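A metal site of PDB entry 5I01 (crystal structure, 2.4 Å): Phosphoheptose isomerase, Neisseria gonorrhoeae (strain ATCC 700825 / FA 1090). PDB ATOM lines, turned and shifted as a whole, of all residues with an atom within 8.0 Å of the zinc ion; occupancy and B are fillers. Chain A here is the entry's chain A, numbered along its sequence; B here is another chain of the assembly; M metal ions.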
ATOM      1  N   HIS A  63     -13.020   3.073 -15.717  1.00  0.00           N
ATOM      2  CA  HIS A  63     -13.885   3.986 -14.938  1.00  0.00           C
ATOM      3  C   HIS A  63     -15.332   3.950 -15.485  1.00  0.00           C
ATOM      4  O   HIS A  63     -16.279   3.753 -14.733  1.00  0.00           O
ATOM      5  CB  HIS A  63     -13.326   5.414 -15.031  1.00  0.00           C
ATOM      6  CG  HIS A  63     -13.974   6.422 -14.120  1.00  0.00           C
ATOM      7  ND1 HIS A  63     -13.247   7.413 -13.495  1.00  0.00           N
ATOM      8  CD2 HIS A  63     -15.264   6.627 -13.761  1.00  0.00           C
ATOM      9  CE1 HIS A  63     -14.056   8.176 -12.780  1.00  0.00           C
ATOM     10  NE2 HIS A  63     -15.285   7.718 -12.921  1.00  0.00           N
ATOM     11  N   PHE A  64     -15.484   4.138 -16.798  1.00  0.00           N
ATOM     12  CA  PHE A  64     -16.787   3.999 -17.472  1.00  0.00           C
ATOM     13  C   PHE A  64     -17.472   2.654 -17.194  1.00  0.00           C
ATOM     14  O   PHE A  64     -18.589   2.612 -16.759  1.00  0.00           O
ATOM     15  CB  PHE A  64     -16.623   4.186 -18.963  1.00  0.00           C
ATOM     16  CG  PHE A  64     -17.843   3.836 -19.747  1.00  0.00           C
ATOM     17  CD1 PHE A  64     -18.999   4.598 -19.623  1.00  0.00           C
ATOM     18  CD2 PHE A  64     -17.849   2.726 -20.593  1.00  0.00           C
ATOM     19  CE1 PHE A  64     -20.141   4.266 -20.344  1.00  0.00           C
ATOM     20  CE2 PHE A  64     -18.980   2.387 -21.308  1.00  0.00           C
ATOM     21  CZ  PHE A  64     -20.125   3.162 -21.189  1.00  0.00           C
ATOM     22  N   ALA A  66     -16.870   0.413 -14.848  1.00  0.00           N
ATOM     23  CA  ALA A  66     -17.157   0.238 -13.423  1.00  0.00           C
ATOM     24  C   ALA A  66     -18.432   0.971 -12.950  1.00  0.00           C
ATOM     25  O   ALA A  66     -19.164   0.481 -12.084  1.00  0.00           O
ATOM     26  CB  ALA A  66     -15.963   0.661 -12.582  1.00  0.00           C
ATOM     27  N   GLU A  67     -18.716   2.147 -13.521  1.00  0.00           N
ATOM     28  CA  GLU A  67     -19.970   2.844 -13.214  1.00  0.00           C
ATOM     29  C   GLU A  67     -21.221   2.210 -13.875  1.00  0.00           C
ATOM     30  O   GLU A  67     -22.327   2.403 -13.410  1.00  0.00           O
ATOM     31  CB  GLU A  67     -19.845   4.330 -13.511  1.00  0.00           C
ATOM     32  CG  GLU A  67     -18.923   5.005 -12.501  1.00  0.00           C
ATOM     33  CD  GLU A  67     -18.874   6.515 -12.619  1.00  0.00           C
ATOM     34  OE1 GLU A  67     -19.204   7.029 -13.700  1.00  0.00           O
ATOM     35  OE2 GLU A  67     -18.503   7.166 -11.630  1.00  0.00           O
ATOM     36  N   ILE A 181     -13.705  12.549 -19.274  1.00  0.00           N
ATOM     37  CA  ILE A 181     -14.324  11.986 -18.067  1.00  0.00           C
ATOM     38  C   ILE A 181     -15.634  12.705 -17.723  1.00  0.00           C
ATOM     39  O   ILE A 181     -16.580  12.074 -17.274  1.00  0.00           O
ATOM     40  CB  ILE A 181     -13.355  11.897 -16.856  1.00  0.00           C
ATOM     41  CG1 ILE A 181     -13.896  10.939 -15.805  1.00  0.00           C
ATOM     42  CG2 ILE A 181     -13.070  13.251 -16.225  1.00  0.00           C
ATOM     43  CD1 ILE A 181     -13.961   9.495 -16.288  1.00  0.00           C
ATOM     44  N   ILE A 184     -18.137  11.174 -20.197  1.00  0.00           N
ATOM     45  CA  ILE A 184     -18.539   9.863 -19.666  1.00  0.00           C
ATOM     46  C   ILE A 184     -19.585   9.987 -18.572  1.00  0.00           C
ATOM     47  O   ILE A 184     -20.585   9.282 -18.588  1.00  0.00           O
ATOM     48  CB  ILE A 184     -17.311   9.063 -19.175  1.00  0.00           C
ATOM     49  CG1 ILE A 184     -16.576   8.507 -20.403  1.00  0.00           C
ATOM     50  CG2 ILE A 184     -17.702   7.958 -18.200  1.00  0.00           C
ATOM     51  CD1 ILE A 184     -15.189   7.962 -20.120  1.00  0.00           C
ATOM     52  N   HIS A 185     -19.339  10.882 -17.617  1.00  0.00           N
ATOM     53  CA  HIS A 185     -20.255  11.116 -16.494  1.00  0.00           C
ATOM     54  C   HIS A 185     -21.623  11.591 -16.958  1.00  0.00           C
ATOM     55  O   HIS A 185     -22.631  11.129 -16.446  1.00  0.00           O
ATOM     56  CB  HIS A 185     -19.653  12.103 -15.485  1.00  0.00           C
ATOM     57  CG  HIS A 185     -18.642  11.484 -14.590  1.00  0.00           C
ATOM     58  ND1 HIS A 185     -17.622  12.204 -14.002  1.00  0.00           N
ATOM     59  CD2 HIS A 185     -18.463  10.195 -14.197  1.00  0.00           C
ATOM     60  CE1 HIS A 185     -16.882  11.391 -13.254  1.00  0.00           C
ATOM     61  NE2 HIS A 185     -17.365  10.165 -13.366  1.00  0.00           N
ATOM     62  N   CYS A 188     -23.416   8.499 -18.603  1.00  0.00           N
ATOM     63  CA  CYS A 188     -23.916   7.594 -17.548  1.00  0.00           C
ATOM     64  C   CYS A 188     -25.136   8.124 -16.822  1.00  0.00           C
ATOM     65  O   CYS A 188     -26.033   7.356 -16.489  1.00  0.00           O
ATOM     66  CB  CYS A 188     -22.842   7.315 -16.492  1.00  0.00           C
ATOM     67  SG  CYS A 188     -21.399   6.458 -17.137  1.00  0.00           S
ATOM     68  N   GLY B  55     -13.112   2.670  -6.919  1.00  0.00           N
ATOM     69  CA  GLY B  55     -13.944   3.064  -8.064  1.00  0.00           C
ATOM     70  C   GLY B  55     -13.148   3.889  -9.053  1.00  0.00           C
ATOM     71  O   GLY B  55     -12.023   3.526  -9.417  1.00  0.00           O
ATOM     72  N   GLY B  56     -13.735   5.018  -9.441  1.00  0.00           N
ATOM     73  CA  GLY B  56     -13.051   6.001 -10.268  1.00  0.00           C
ATOM     74  C   GLY B  56     -11.734   6.496  -9.690  1.00  0.00           C
ATOM     75  O   GLY B  56     -10.846   6.886 -10.436  1.00  0.00           O
ATOM     76  N   SER B  57     -11.614   6.500  -8.353  1.00  0.00           N
ATOM     77  CA  SER B  57     -10.377   6.921  -7.710  1.00  0.00           C
ATOM     78  C   SER B  57      -9.265   5.872  -7.862  1.00  0.00           C
ATOM     79  O   SER B  57      -8.090   6.214  -7.785  1.00  0.00           O
ATOM     80  CB  SER B  57     -10.638   7.278  -6.246  1.00  0.00           C
ATOM     81  OG  SER B  57     -11.641   8.286  -6.145  1.00  0.00           O
ATOM     82  N   ASP B  60      -7.949   6.819 -11.174  1.00  0.00           N
ATOM     83  CA  ASP B  60      -7.085   8.002 -10.975  1.00  0.00           C
ATOM     84  C   ASP B  60      -5.723   7.656 -10.379  1.00  0.00           C
ATOM     85  O   ASP B  60      -4.728   8.248 -10.751  1.00  0.00           O
ATOM     86  CB  ASP B  60      -7.777   9.085 -10.113  1.00  0.00           C
ATOM     87  CG  ASP B  60      -9.120   9.589 -10.726  1.00  0.00           C
ATOM     88  OD1 ASP B  60      -9.314   9.464 -11.960  1.00  0.00           O
ATOM     89  OD2 ASP B  60      -9.983  10.113  -9.973  1.00  0.00           O
ATOM     90  N   THR B 123     -13.477  10.153  -2.489  1.00  0.00           N
ATOM     91  CA  THR B 123     -14.401  11.268  -2.773  1.00  0.00           C
ATOM     92  C   THR B 123     -15.140  11.846  -1.534  1.00  0.00           C
ATOM     93  O   THR B 123     -15.434  13.045  -1.494  1.00  0.00           O
ATOM     94  CB  THR B 123     -15.441  10.896  -3.858  1.00  0.00           C
ATOM     95  OG1 THR B 123     -16.084   9.677  -3.501  1.00  0.00           O
ATOM     96  CG2 THR B 123     -14.756  10.737  -5.220  1.00  0.00           C
ATOM     97  N   THR B 173     -20.093  13.384  -6.482  1.00  0.00           N
ATOM     98  CA  THR B 173     -18.927  12.531  -6.686  1.00  0.00           C
ATOM     99  C   THR B 173     -18.251  12.712  -8.063  1.00  0.00           C
ATOM    100  O   THR B 173     -17.026  12.732  -8.158  1.00  0.00           O
ATOM    101  CB  THR B 173     -19.327  11.044  -6.482  1.00  0.00           C
ATOM    102  OG1 THR B 173     -19.702  10.849  -5.103  1.00  0.00           O
ATOM    103  CG2 THR B 173     -18.189  10.067  -6.864  1.00  0.00           C
ATOM    104  N   ALA B 174     -19.060  12.822  -9.111  1.00  0.00           N
ATOM    105  CA  ALA B 174     -18.556  13.096 -10.464  1.00  0.00           C
ATOM    106  C   ALA B 174     -17.705  14.375 -10.543  1.00  0.00           C
ATOM    107  O   ALA B 174     -16.643  14.399 -11.169  1.00  0.00           O
ATOM    108  CB  ALA B 174     -19.705  13.155 -11.459  1.00  0.00           C
ATOM    109  N   ARG B 175     -18.175  15.437  -9.896  1.00  0.00           N
ATOM    110  CA  ARG B 175     -17.479  16.727  -9.895  1.00  0.00           C
ATOM    111  C   ARG B 175     -16.168  16.664  -9.107  1.00  0.00           C
ATOM    112  O   ARG B 175     -15.188  17.305  -9.462  1.00  0.00           O
ATOM    113  CB  ARG B 175     -18.384  17.809  -9.336  1.00  0.00           C
ATOM    114  CG  ARG B 175     -19.692  18.023 -10.094  1.00  0.00           C
ATOM    115  CD  ARG B 175     -19.473  18.581 -11.486  1.00  0.00           C
ATOM    116  NE  ARG B 175     -19.312  17.527 -12.484  1.00  0.00           N
ATOM    117  CZ  ARG B 175     -20.313  16.826 -13.036  1.00  0.00           C
ATOM    118  NH1 ARG B 175     -20.040  15.897 -13.946  1.00  0.00           N
ATOM    119  NH2 ARG B 175     -21.581  17.056 -12.685  1.00  0.00           N
ATOM    120  N   GLN B 177     -14.327  13.880  -8.687  1.00  0.00           N
ATOM    121  CA  GLN B 177     -13.426  13.066  -9.498  1.00  0.00           C
ATOM    122  C   GLN B 177     -12.766  13.907 -10.573  1.00  0.00           C
ATOM    123  O   GLN B 177     -11.549  13.900 -10.698  1.00  0.00           O
ATOM    124  CB  GLN B 177     -14.160  11.873 -10.138  1.00  0.00           C
ATOM    125  CG  GLN B 177     -14.489  10.800  -9.122  1.00  0.00           C
ATOM    126  CD  GLN B 177     -15.330   9.654  -9.661  1.00  0.00           C
ATOM    127  OE1 GLN B 177     -15.971   9.747 -10.709  1.00  0.00           O
ATOM    128  NE2 GLN B 177     -15.338   8.547  -8.928  1.00  0.00           N
ATOM    129  N   GLU B 178     -13.571  14.639 -11.331  1.00  0.00           N
ATOM    130  CA  GLU B 178     -13.081  15.507 -12.407  1.00  0.00           C
ATOM    131  C   GLU B 178     -12.007  16.469 -11.916  1.00  0.00           C
ATOM    132  O   GLU B 178     -10.989  16.656 -12.564  1.00  0.00           O
ATOM    133  CB  GLU B 178     -14.231  16.279 -13.039  1.00  0.00           C
ATOM    134  CG  GLU B 178     -15.142  15.397 -13.897  1.00  0.00           C
ATOM    135  CD  GLU B 178     -16.603  15.858 -13.946  1.00  0.00           C
ATOM    136  OE1 GLU B 178     -16.902  17.032 -13.600  1.00  0.00           O
ATOM    137  OE2 GLU B 178     -17.468  15.008 -14.321  1.00  0.00           O
ATOM    138  N   ILE B 181      -8.499  14.637 -11.090  1.00  0.00           N
ATOM    139  CA  ILE B 181      -7.687  14.347 -12.270  1.00  0.00           C
ATOM    140  C   ILE B 181      -7.008  15.637 -12.720  1.00  0.00           C
ATOM    141  O   ILE B 181      -5.852  15.611 -13.121  1.00  0.00           O
ATOM    142  CB  ILE B 181      -8.493  13.694 -13.431  1.00  0.00           C
ATOM    143  CG1 ILE B 181      -9.196  12.408 -12.985  1.00  0.00           C
ATOM    144  CG2 ILE B 181      -7.557  13.296 -14.572  1.00  0.00           C
ATOM    145  CD1 ILE B 181     -10.390  11.985 -13.826  1.00  0.00           C
HETATM  146 ZN    ZN M   1     -17.027   8.532 -11.911  1.00  0.00          ZN
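O of Ile 181 of chain A sits close to ND1 of His 185 (3.4 Å). A ring nitrogen (ND1) of His 185 lies within hydrogen-bond range of the side-chain carboxylate (OE2) of Glu 178 of chain B (2.8 Å).
Within 4 Å of the zinc ion: His 63, Glu 67, His 185 and Gln 177 of chain B. The nearest printed residue that does not touch the zinc ion is Gly 56 of chain B (5.0 Å).
The zinc ion is bound by the side-chain amide oxygen of Gln 177 of chain B (2.0 Å), the side-chain carboxylate of Glu 67 (2.0 Å), a ring nitrogen (NE2) of His 63 (2.2 Å) and a ring nitrogen (NE2) of His 185 (2.2 Å). The zinc ion has four donor atoms within binding distance.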
